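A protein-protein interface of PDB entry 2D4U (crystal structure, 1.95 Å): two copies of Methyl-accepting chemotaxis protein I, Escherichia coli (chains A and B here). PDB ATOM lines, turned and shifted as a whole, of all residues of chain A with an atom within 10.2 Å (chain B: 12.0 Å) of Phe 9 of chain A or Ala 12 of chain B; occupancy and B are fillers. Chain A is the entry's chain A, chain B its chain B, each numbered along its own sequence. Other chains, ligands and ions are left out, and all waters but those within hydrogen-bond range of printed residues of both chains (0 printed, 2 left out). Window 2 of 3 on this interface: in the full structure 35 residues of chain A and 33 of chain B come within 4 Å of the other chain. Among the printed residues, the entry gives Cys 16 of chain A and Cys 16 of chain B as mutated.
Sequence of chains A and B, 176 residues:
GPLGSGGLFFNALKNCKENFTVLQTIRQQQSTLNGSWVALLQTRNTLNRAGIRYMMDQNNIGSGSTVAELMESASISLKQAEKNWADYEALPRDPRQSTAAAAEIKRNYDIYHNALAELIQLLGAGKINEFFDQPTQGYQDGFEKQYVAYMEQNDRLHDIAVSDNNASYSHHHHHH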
ATOM      1  N   LEU A   3      40.985  20.473 -15.784  1.00  0.00           N
ATOM      2  CA  LEU A   3      40.393  20.157 -14.496  1.00  0.00           C
ATOM      3  C   LEU A   3      39.259  19.174 -14.789  1.00  0.00           C
ATOM      4  O   LEU A   3      38.537  19.375 -15.743  1.00  0.00           O
ATOM      5  CB  LEU A   3      39.818  21.429 -13.888  1.00  0.00           C
ATOM      6  CG  LEU A   3      40.006  21.693 -12.394  1.00  0.00           C
ATOM      7  CD1 LEU A   3      38.813  22.471 -11.842  1.00  0.00           C
ATOM      8  CD2 LEU A   3      40.199  20.402 -11.632  1.00  0.00           C
ATOM      9  N   GLY A   4      39.101  18.132 -13.971  1.00  0.00           N
ATOM     10  CA  GLY A   4      38.079  17.114 -14.166  1.00  0.00           C
ATOM     11  C   GLY A   4      36.658  17.442 -13.703  1.00  0.00           C
ATOM     12  O   GLY A   4      36.431  18.466 -13.082  1.00  0.00           O
ATOM     13  N   SER A   5      35.697  16.565 -14.015  1.00  0.00           N
ATOM     14  CA  SER A   5      34.296  16.748 -13.608  1.00  0.00           C
ATOM     15  C   SER A   5      34.142  16.762 -12.091  1.00  0.00           C
ATOM     16  O   SER A   5      33.375  17.562 -11.542  1.00  0.00           O
ATOM     17  CB  SER A   5      33.401  15.653 -14.200  1.00  0.00           C
ATOM     18  OG  SER A   5      33.658  15.464 -15.582  1.00  0.00           O
ATOM     19  N   GLY A   6      34.863  15.866 -11.422  1.00  0.00           N
ATOM     20  CA  GLY A   6      34.811  15.795  -9.982  1.00  0.00           C
ATOM     21  C   GLY A   6      35.209  17.140  -9.409  1.00  0.00           C
ATOM     22  O   GLY A   6      34.536  17.686  -8.528  1.00  0.00           O
ATOM     23  N   GLY A   7      36.311  17.685  -9.913  1.00  0.00           N
ATOM     24  CA  GLY A   7      36.765  18.985  -9.463  1.00  0.00           C
ATOM     25  C   GLY A   7      35.805  20.114  -9.795  1.00  0.00           C
ATOM     26  O   GLY A   7      35.538  20.975  -8.953  1.00  0.00           O
ATOM     27  N   LEU A   8      35.305  20.133 -11.023  1.00  0.00           N
ATOM     28  CA  LEU A   8      34.387  21.183 -11.431  1.00  0.00           C
ATOM     29  C   LEU A   8      33.198  21.178 -10.486  1.00  0.00           C
ATOM     30  O   LEU A   8      32.714  22.238 -10.077  1.00  0.00           O
ATOM     31  CB  LEU A   8      33.933  21.003 -12.881  1.00  0.00           C
ATOM     32  CG  LEU A   8      35.028  21.246 -13.938  1.00  0.00           C
ATOM     33  CD1 LEU A   8      34.588  20.892 -15.394  1.00  0.00           C
ATOM     34  CD2 LEU A   8      35.508  22.701 -13.872  1.00  0.00           C
ATOM     35  N   PHE A   9      32.741  19.976 -10.137  1.00  0.00           N
ATOM     36  CA  PHE A   9      31.597  19.786  -9.255  1.00  0.00           C
ATOM     37  C   PHE A   9      31.899  20.276  -7.859  1.00  0.00           C
ATOM     38  O   PHE A   9      31.101  20.962  -7.260  1.00  0.00           O
ATOM     39  CB  PHE A   9      31.219  18.313  -9.184  1.00  0.00           C
ATOM     40  CG  PHE A   9      30.137  17.995  -8.177  1.00  0.00           C
ATOM     41  CD1 PHE A   9      30.461  17.764  -6.845  1.00  0.00           C
ATOM     42  CD2 PHE A   9      28.811  17.884  -8.567  1.00  0.00           C
ATOM     43  CE1 PHE A   9      29.483  17.451  -5.912  1.00  0.00           C
ATOM     44  CE2 PHE A   9      27.825  17.560  -7.634  1.00  0.00           C
ATOM     45  CZ  PHE A   9      28.174  17.350  -6.297  1.00  0.00           C
ATOM     46  N   PHE A  10      33.046  19.902  -7.332  1.00  0.00           N
ATOM     47  CA  PHE A  10      33.401  20.344  -5.997  1.00  0.00           C
ATOM     48  C   PHE A  10      33.483  21.884  -5.907  1.00  0.00           C
ATOM     49  O   PHE A  10      32.969  22.509  -4.970  1.00  0.00           O
ATOM     50  CB  PHE A  10      34.724  19.715  -5.607  1.00  0.00           C
ATOM     51  CG  PHE A  10      35.176  20.068  -4.229  1.00  0.00           C
ATOM     52  CD1 PHE A  10      34.790  19.307  -3.148  1.00  0.00           C
ATOM     53  CD2 PHE A  10      36.001  21.155  -4.027  1.00  0.00           C
ATOM     54  CE1 PHE A  10      35.223  19.642  -1.873  1.00  0.00           C
ATOM     55  CE2 PHE A  10      36.438  21.498  -2.760  1.00  0.00           C
ATOM     56  CZ  PHE A  10      36.052  20.741  -1.683  1.00  0.00           C
ATOM     57  N   ASN A  11      34.122  22.483  -6.901  1.00  0.00           N
ATOM     58  CA  ASN A  11      34.256  23.924  -6.952  1.00  0.00           C
ATOM     59  C   ASN A  11      32.916  24.628  -7.120  1.00  0.00           C
ATOM     60  O   ASN A  11      32.679  25.665  -6.498  1.00  0.00           O
ATOM     61  CB  ASN A  11      35.190  24.326  -8.092  1.00  0.00           C
ATOM     62  CG  ASN A  11      35.122  25.806  -8.401  1.00  0.00           C
ATOM     63  OD1 ASN A  11      34.916  26.209  -9.549  1.00  0.00           O
ATOM     64  ND2 ASN A  11      35.281  26.633  -7.368  1.00  0.00           N
ATOM     65  N   ALA A  12      32.048  24.079  -7.967  1.00  0.00           N
ATOM     66  CA  ALA A  12      30.721  24.660  -8.153  1.00  0.00           C
ATOM     67  C   ALA A  12      29.906  24.564  -6.875  1.00  0.00           C
ATOM     68  O   ALA A  12      29.194  25.502  -6.516  1.00  0.00           O
ATOM     69  CB  ALA A  12      29.979  24.001  -9.309  1.00  0.00           C
ATOM     70  N   LEU A  13      30.015  23.437  -6.183  1.00  0.00           N
ATOM     71  CA  LEU A  13      29.254  23.237  -4.953  1.00  0.00           C
ATOM     72  C   LEU A  13      29.773  24.155  -3.836  1.00  0.00           C
ATOM     73  O   LEU A  13      28.985  24.660  -3.021  1.00  0.00           O
ATOM     74  CB  LEU A  13      29.314  21.783  -4.504  1.00  0.00           C
ATOM     75  CG  LEU A  13      28.117  21.158  -3.767  1.00  0.00           C
ATOM     76  CD1 LEU A  13      28.583  20.091  -2.815  1.00  0.00           C
ATOM     77  CD2 LEU A  13      27.260  22.162  -3.015  1.00  0.00           C
ATOM     78  N   LYS A  14      31.093  24.362  -3.811  1.00  0.00           N
ATOM     79  CA  LYS A  14      31.748  25.235  -2.837  1.00  0.00           C
ATOM     80  C   LYS A  14      31.215  26.648  -2.982  1.00  0.00           C
ATOM     81  O   LYS A  14      30.799  27.267  -2.002  1.00  0.00           O
ATOM     82  CB  LYS A  14      33.259  25.258  -3.068  1.00  0.00           C
ATOM     83  CG  LYS A  14      34.115  25.779  -1.892  1.00  0.00           C
ATOM     84  CD  LYS A  14      35.595  25.817  -2.304  1.00  0.00           C
ATOM     85  CE  LYS A  14      36.532  25.429  -1.167  1.00  0.00           C
ATOM     86  NZ  LYS A  14      37.590  24.460  -1.623  1.00  0.00           N
ATOM     87  N   ASN A  15      31.251  27.154  -4.212  1.00  0.00           N
ATOM     88  CA  ASN A  15      30.792  28.497  -4.499  1.00  0.00           C
ATOM     89  C   ASN A  15      29.302  28.657  -4.239  1.00  0.00           C
ATOM     90  O   ASN A  15      28.879  29.653  -3.681  1.00  0.00           O
ATOM     91  CB  ASN A  15      31.107  28.904  -5.941  1.00  0.00           C
ATOM     92  CG  ASN A  15      32.486  29.557  -6.082  1.00  0.00           C
ATOM     93  OD1 ASN A  15      33.242  29.701  -5.105  1.00  0.00           O
ATOM     94  ND2 ASN A  15      32.816  29.957  -7.302  1.00  0.00           N
ATOM     95  N   CYS A  16      28.514  27.678  -4.658  1.00  0.00           N
ATOM     96  CA  CYS A  16      27.071  27.758  -4.457  1.00  0.00           C
ATOM     97  C   CYS A  16      26.747  27.897  -2.985  1.00  0.00           C
ATOM     98  O   CYS A  16      25.934  28.725  -2.585  1.00  0.00           O
ATOM     99  CB  CYS A  16      26.348  26.540  -5.035  1.00  0.00           C
ATOM    100  SG  CYS A  16      24.549  26.598  -4.782  1.00  0.00           S
ATOM    101  N   LYS A  17      27.401  27.080  -2.180  1.00  0.00           N
ATOM    102  CA  LYS A  17      27.152  27.054  -0.764  1.00  0.00           C
ATOM    103  C   LYS A  17      27.590  28.374  -0.121  1.00  0.00           C
ATOM    104  O   LYS A  17      27.042  28.785   0.895  1.00  0.00           O
ATOM    105  CB  LYS A  17      27.885  25.873  -0.152  1.00  0.00           C
ATOM    106  CG  LYS A  17      27.080  25.135   0.900  1.00  0.00           C
ATOM    107  CD  LYS A  17      27.558  23.705   1.090  1.00  0.00           C
ATOM    108  CE  LYS A  17      27.001  23.144   2.390  1.00  0.00           C
ATOM    109  NZ  LYS A  17      27.308  21.693   2.613  1.00  0.00           N
ATOM    110  N   PHE A  20      24.845  30.956  -1.306  1.00  0.00           N
ATOM    111  CA  PHE A  20      23.624  30.759  -0.575  1.00  0.00           C
ATOM    112  C   PHE A  20      23.699  31.392   0.806  1.00  0.00           C
ATOM    113  O   PHE A  20      22.768  32.079   1.239  1.00  0.00           O
ATOM    114  CB  PHE A  20      23.363  29.288  -0.427  1.00  0.00           C
ATOM    115  CG  PHE A  20      22.103  28.992   0.247  1.00  0.00           C
ATOM    116  CD1 PHE A  20      22.057  28.884   1.618  1.00  0.00           C
ATOM    117  CD2 PHE A  20      20.945  28.833  -0.488  1.00  0.00           C
ATOM    118  CE1 PHE A  20      20.848  28.612   2.249  1.00  0.00           C
ATOM    119  CE2 PHE A  20      19.767  28.544   0.132  1.00  0.00           C
ATOM    120  CZ  PHE A  20      19.717  28.445   1.498  1.00  0.00           C
ATOM    121  N   ASN A 165      26.600  32.732  -9.134  1.00  0.00           N
ATOM    122  CA  ASN A 165      25.795  31.538  -9.325  1.00  0.00           C
ATOM    123  C   ASN A 165      25.478  31.289 -10.786  1.00  0.00           C
ATOM    124  O   ASN A 165      25.407  30.143 -11.219  1.00  0.00           O
ATOM    125  CB  ASN A 165      24.501  31.624  -8.520  1.00  0.00           C
ATOM    126  CG  ASN A 165      23.611  30.407  -8.716  1.00  0.00           C
ATOM    127  OD1 ASN A 165      23.882  29.332  -8.177  1.00  0.00           O
ATOM    128  ND2 ASN A 165      22.540  30.573  -9.488  1.00  0.00           N
ATOM    129  N   ASN B  11      21.273  15.777  -6.773  1.00  0.00           N
ATOM    130  CA  ASN B  11      22.718  16.133  -6.819  1.00  0.00           C
ATOM    131  C   ASN B  11      22.977  17.177  -5.746  1.00  0.00           C
ATOM    132  O   ASN B  11      22.082  17.945  -5.407  1.00  0.00           O
ATOM    133  CB  ASN B  11      23.095  16.689  -8.192  1.00  0.00           C
ATOM    134  CG  ASN B  11      22.230  16.128  -9.310  1.00  0.00           C
ATOM    135  OD1 ASN B  11      22.619  16.136 -10.480  1.00  0.00           O
ATOM    136  ND2 ASN B  11      21.040  15.644  -8.957  1.00  0.00           N
ATOM    137  N   ALA B  12      24.176  17.203  -5.185  1.00  0.00           N
ATOM    138  CA  ALA B  12      24.475  18.220  -4.191  1.00  0.00           C
ATOM    139  C   ALA B  12      24.438  19.577  -4.877  1.00  0.00           C
ATOM    140  O   ALA B  12      23.940  20.550  -4.322  1.00  0.00           O
ATOM    141  CB  ALA B  12      25.822  17.981  -3.554  1.00  0.00           C
ATOM    142  N   LEU B  13      24.927  19.619  -6.110  1.00  0.00           N
ATOM    143  CA  LEU B  13      25.018  20.867  -6.848  1.00  0.00           C
ATOM    144  C   LEU B  13      23.666  21.408  -7.321  1.00  0.00           C
ATOM    145  O   LEU B  13      23.271  22.499  -6.927  1.00  0.00           O
ATOM    146  CB  LEU B  13      25.985  20.719  -8.021  1.00  0.00           C
ATOM    147  CG  LEU B  13      26.231  21.982  -8.836  1.00  0.00           C
ATOM    148  CD1 LEU B  13      26.818  23.092  -7.965  1.00  0.00           C
ATOM    149  CD2 LEU B  13      27.141  21.669 -10.013  1.00  0.00           C
ATOM    150  N   LYS B  14      22.961  20.660  -8.166  1.00  0.00           N
ATOM    151  CA  LYS B  14      21.654  21.119  -8.650  1.00  0.00           C
ATOM    152  C   LYS B  14      20.706  21.416  -7.495  1.00  0.00           C
ATOM    153  O   LYS B  14      19.797  22.226  -7.613  1.00  0.00           O
ATOM    154  CB  LYS B  14      21.031  20.122  -9.638  1.00  0.00           C
ATOM    155  CG  LYS B  14      21.128  20.559 -11.110  1.00  0.00           C
ATOM    156  CD  LYS B  14      22.552  20.994 -11.498  1.00  0.00           C
ATOM    157  CE  LYS B  14      22.578  21.757 -12.828  1.00  0.00           C
ATOM    158  NZ  LYS B  14      23.953  22.233 -13.149  1.00  0.00           N
ATOM    159  N   ASN B  15      20.935  20.761  -6.369  1.00  0.00           N
ATOM    160  CA  ASN B  15      20.138  20.988  -5.183  1.00  0.00           C
ATOM    161  C   ASN B  15      20.393  22.394  -4.638  1.00  0.00           C
ATOM    162  O   ASN B  15      19.479  23.097  -4.187  1.00  0.00           O
ATOM    163  CB  ASN B  15      20.547  19.982  -4.115  1.00  0.00           C
ATOM    164  CG  ASN B  15      19.404  19.581  -3.217  1.00  0.00           C
ATOM    165  OD1 ASN B  15      18.562  18.771  -3.600  1.00  0.00           O
ATOM    166  ND2 ASN B  15      19.371  20.132  -2.010  1.00  0.00           N
ATOM    167  N   CYS B  16      21.653  22.797  -4.678  1.00  0.00           N
ATOM    168  CA  CYS B  16      22.049  24.070  -4.115  1.00  0.00           C
ATOM    169  C   CYS B  16      21.720  25.185  -5.086  1.00  0.00           C
ATOM    170  O   CYS B  16      21.311  26.271  -4.686  1.00  0.00           O
ATOM    171  CB  CYS B  16      23.538  24.036  -3.741  1.00  0.00           C
ATOM    172  SG  CYS B  16      24.226  25.587  -3.110  1.00  0.00           S
ATOM    173  N   LYS B  17      21.875  24.909  -6.370  1.00  0.00           N
ATOM    174  CA  LYS B  17      21.573  25.893  -7.391  1.00  0.00           C
ATOM    175  C   LYS B  17      20.075  26.233  -7.354  1.00  0.00           C
ATOM    176  O   LYS B  17      19.672  27.329  -7.747  1.00  0.00           O
ATOM    177  CB  LYS B  17      21.978  25.372  -8.770  1.00  0.00           C
ATOM    178  CG  LYS B  17      23.484  25.126  -8.971  1.00  0.00           C
ATOM    179  CD  LYS B  17      24.084  26.019 -10.071  1.00  0.00           C
ATOM    180  CE  LYS B  17      25.097  25.238 -10.938  1.00  0.00           C
ATOM    181  NZ  LYS B  17      25.600  25.997 -12.137  1.00  0.00           N
ATOM    182  N   GLU B  18      19.249  25.300  -6.877  1.00  0.00           N
ATOM    183  CA  GLU B  18      17.808  25.550  -6.813  1.00  0.00           C
ATOM    184  C   GLU B  18      17.439  26.196  -5.480  1.00  0.00           C
ATOM    185  O   GLU B  18      16.542  27.024  -5.411  1.00  0.00           O
ATOM    186  CB  GLU B  18      16.998  24.273  -7.042  1.00  0.00           C
ATOM    187  CG  GLU B  18      16.383  23.695  -5.776  1.00  0.00           C
ATOM    188  CD  GLU B  18      15.741  22.327  -5.984  1.00  0.00           C
ATOM    189  OE1 GLU B  18      15.816  21.774  -7.111  1.00  0.00           O
ATOM    190  OE2 GLU B  18      15.159  21.796  -5.009  1.00  0.00           O
ATOM    191  N   ASN B  19      18.138  25.814  -4.422  1.00  0.00           N
ATOM    192  CA  ASN B  19      17.914  26.410  -3.119  1.00  0.00           C
ATOM    193  C   ASN B  19      18.243  27.899  -3.133  1.00  0.00           C
ATOM    194  O   ASN B  19      17.585  28.697  -2.467  1.00  0.00           O
ATOM    195  CB  ASN B  19      18.778  25.720  -2.083  1.00  0.00           C
ATOM    196  CG  ASN B  19      18.087  24.547  -1.440  1.00  0.00           C
ATOM    197  OD1 ASN B  19      17.085  24.028  -1.951  1.00  0.00           O
ATOM    198  ND2 ASN B  19      18.612  24.125  -0.293  1.00  0.00           N
ATOM    199  N   PHE B  20      19.277  28.253  -3.892  1.00  0.00           N
ATOM    200  CA  PHE B  20      19.711  29.623  -4.033  1.00  0.00           C
ATOM    201  C   PHE B  20      18.637  30.386  -4.817  1.00  0.00           C
ATOM    202  O   PHE B  20      18.328  31.539  -4.509  1.00  0.00           O
ATOM    203  CB  PHE B  20      21.081  29.663  -4.730  1.00  0.00           C
ATOM    204  CG  PHE B  20      21.471  31.014  -5.231  1.00  0.00           C
ATOM    205  CD1 PHE B  20      20.962  31.490  -6.426  1.00  0.00           C
ATOM    206  CD2 PHE B  20      22.362  31.802  -4.528  1.00  0.00           C
ATOM    207  CE1 PHE B  20      21.307  32.737  -6.906  1.00  0.00           C
ATOM    208  CE2 PHE B  20      22.720  33.067  -5.013  1.00  0.00           C
ATOM    209  CZ  PHE B  20      22.181  33.522  -6.201  1.00  0.00           C
ATOM    210  N   THR B  21      18.039  29.725  -5.804  1.00  0.00           N
ATOM    211  CA  THR B  21      16.996  30.361  -6.601  1.00  0.00           C
ATOM    212  C   THR B  21      15.782  30.721  -5.743  1.00  0.00           C
ATOM    213  O   THR B  21      15.130  31.762  -5.933  1.00  0.00           O
ATOM    214  CB  THR B  21      16.581  29.456  -7.757  1.00  0.00           C
ATOM    215  OG1 THR B  21      17.628  29.435  -8.735  1.00  0.00           O
ATOM    216  CG2 THR B  21      15.414  30.078  -8.522  1.00  0.00           C
ATOM    217  N   ILE B 160      13.631  25.588   4.542  1.00  0.00           N
ATOM    218  CA  ILE B 160      13.832  24.318   3.847  1.00  0.00           C
ATOM    219  C   ILE B 160      15.053  24.421   2.967  1.00  0.00           C
ATOM    220  O   ILE B 160      15.752  23.436   2.722  1.00  0.00           O
ATOM    221  CB  ILE B 160      12.591  23.872   3.029  1.00  0.00           C
ATOM    222  CG1 ILE B 160      12.332  24.814   1.845  1.00  0.00           C
ATOM    223  CG2 ILE B 160      11.372  23.713   3.944  1.00  0.00           C
ATOM    224  CD1 ILE B 160      13.093  24.439   0.589  1.00  0.00           C
ATOM    225  N   ALA B 161      15.330  25.628   2.507  1.00  0.00           N
ATOM    226  CA  ALA B 161      16.461  25.803   1.630  1.00  0.00           C
ATOM    227  C   ALA B 161      17.739  25.715   2.438  1.00  0.00           C
ATOM    228  O   ALA B 161      18.725  25.142   1.984  1.00  0.00           O
ATOM    229  CB  ALA B 161      16.368  27.113   0.908  1.00  0.00           C
ATOM    230  N   VAL B 162      17.723  26.264   3.646  1.00  0.00           N
ATOM    231  CA  VAL B 162      18.926  26.232   4.461  1.00  0.00           C
ATOM    232  C   VAL B 162      19.263  24.769   4.747  1.00  0.00           C
ATOM    233  O   VAL B 162      20.427  24.385   4.816  1.00  0.00           O
ATOM    234  CB  VAL B 162      18.777  27.030   5.767  1.00  0.00           C
ATOM    235  CG1 VAL B 162      18.347  28.464   5.484  1.00  0.00           C
ATOM    236  CG2 VAL B 162      17.789  26.366   6.680  1.00  0.00           C
ATOM    237  N   SER B 163      18.226  23.951   4.875  1.00  0.00           N
ATOM    238  CA  SER B 163      18.400  22.532   5.142  1.00  0.00           C
ATOM    239  C   SER B 163      18.991  21.781   3.950  1.00  0.00           C
ATOM    240  O   SER B 163      20.089  21.233   4.037  1.00  0.00           O
ATOM    241  CB  SER B 163      17.063  21.914   5.537  1.00  0.00           C
ATOM    242  OG  SER B 163      16.587  22.509   6.729  1.00  0.00           O
ATOM    243  N   ASP B 164      18.251  21.756   2.847  1.00  0.00           N
ATOM    244  CA  ASP B 164      18.685  21.070   1.633  1.00  0.00           C
ATOM    245  C   ASP B 164      20.127  21.415   1.274  1.00  0.00           C
ATOM    246  O   ASP B 164      20.783  20.703   0.511  1.00  0.00           O
ATOM    247  CB  ASP B 164      17.770  21.433   0.467  1.00  0.00           C
ATOM    248  CG  ASP B 164      16.400  20.808   0.585  1.00  0.00           C
ATOM    249  OD1 ASP B 164      16.028  20.388   1.709  1.00  0.00           O
ATOM    250  OD2 ASP B 164      15.629  20.692  -0.394  1.00  0.00           O
ATOM    251  N   ASN B 165      20.607  22.522   1.824  1.00  0.00           N
ATOM    252  CA  ASN B 165      21.962  22.973   1.574  1.00  0.00           C
ATOM    253  C   ASN B 165      22.998  22.153   2.341  1.00  0.00           C
ATOM    254  O   ASN B 165      23.843  21.474   1.748  1.00  0.00           O
ATOM    255  CB  ASN B 165      22.095  24.436   1.959  1.00  0.00           C
ATOM    256  CG  ASN B 165      23.292  25.089   1.320  1.00  0.00           C
ATOM    257  OD1 ASN B 165      24.106  25.722   1.995  1.00  0.00           O
ATOM    258  ND2 ASN B 165      23.412  24.939  -0.001  1.00  0.00           N
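The side-chain sulfur (SG) of Cys 16 of chain B is disulfide-bonded to the side-chain sulfur (SG) of Cys 16 of chain A, at 2.0 Å.
The side-chain sulfur (SG) of Cys 16 of chain A lies within hydrogen-bond range of the backbone NH (N) of Lys 17 of chain B, at 3.5 Å.
The side-chain sulfur of Cys 16 of chain B is in hydrogen-bond range of the backbone NH of Lys 17 of chain A, at 3.6 Å.
O of Asn 15 of chain B lies close to OD1 of Asn 19 of chain B, at 3.4 Å.
The side-chain amide nitrogen (ND2) of Asn 165 of chain B sits at hydrogen-bond distance from the side-chain sulfur (SG) of Cys 16 of chain B (3.3 Å).
OG1 of Thr 21 of chain B sits at hydrogen-bond distance from O of Lys 17 of chain B.
The side-chain amide nitrogen (ND2) of Asn 19 of chain B is in hydrogen-bond range of the backbone carbonyl oxygen (O) of Ala 161 of chain B (2.5 Å).
The backbone NH of Asn 165 of chain B lies close to the side-chain amide nitrogen of Asn 19 of chain B, 3.3 Å away.
Among the printed residues, pairs that only touch across the chains: Phe 9 of chain A with Ala 12 of chain B, Phe 9 of chain A with Leu 13 of chain B, Ala 12 of chain A with Leu 13 of chain B, Leu 13 of chain A with Ala 12 of chain B, Leu 13 of chain A with Leu 13 of chain B, Lys 17 of chain A with Asn 165 of chain B, Phe 20 of chain A with Asn 19 of chain B, Phe 20 of chain A with Phe 20 of chain B, Phe 20 of chain A with Ala 161 of chain B, Phe 20 of chain A with Val 162 of chain B, Phe 20 of chain A with Asn 165 of chain B, Asn 165 of chain A with Lys 17 of chain B and Asn 165 of chain A with Phe 20 of chain B.
Of the printed residues of chain B, Phe 9 of chain A touches Ala 12 and Leu 13.
Ala 12 of chain B touches two residues of chain A.
No residue of chain B comes within 4 Å of Gly 4 of chain A.
No residue of chain B comes within 4 Å of Ser 5 of chain A.
No residue of chain B comes within 4 Å of Gly 6 of chain A.
No residue of chain B comes within 4 Å of Leu 8 of chain A.
No residue of chain B comes within 4 Å of Phe 10 of chain A.
No residue of chain B comes within 4 Å of Asn 11 of chain A.
Of chain B, only Leu 13 comes within 4 Å of Ala 12 of chain A.
No residue of chain A comes within 4 Å of Asn 11 of chain B.
Of chain A, only Phe 9 (3.7 Å), Ala 12 (3.6 Å) and Leu 13 (3.7 Å) come within 4 Å of Leu 13 of chain B.
Of the printed residues of chain A, Asn 165 of chain B touches Lys 17 and Phe 20.
Printed residues of chain A within 4 Å of Lys 17 of chain B: Cys 16 and Asn 165.
Hydrophobic or aromatic side chains of chain A within 4 Å of the printed part of chain B: Phe 9, Ala 12, Leu 13 and Phe 20.
Along chain A the printed residues that touch a printed residue of chain B span positions 9 to 165.
Of the 17 printed residues of chain B, 9 touch a printed residue of chain A.
Hydrophobic or aromatic side chains of chain B within 4 Å of the printed part of chain A: Ala 12, Leu 13, Phe 20 and Ala 161.
Along chain B the printed residues that touch a printed residue of chain A span positions 12 to 165.
Among the printed residues, no Asp or Glu carboxylate lies within 4 Å of a Lys or Arg side-chain nitrogen of the other chain.
Ala 12 of chain A touches Leu 13 of chain B, and with the chains exchanged Leu 13 of chain A touches Ala 12 of chain B.
Leu 13 of chain A touches its own counterpart, Leu 13 of chain B.
Cys 16 of chain A touches its own counterpart, Cys 16 of chain B.
Phe 20 of chain A touches its own counterpart, Phe 20 of chain B.
Positions printed for both chains: 11, 12, 13, 14, 15, 16, 17, 20 and 165.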
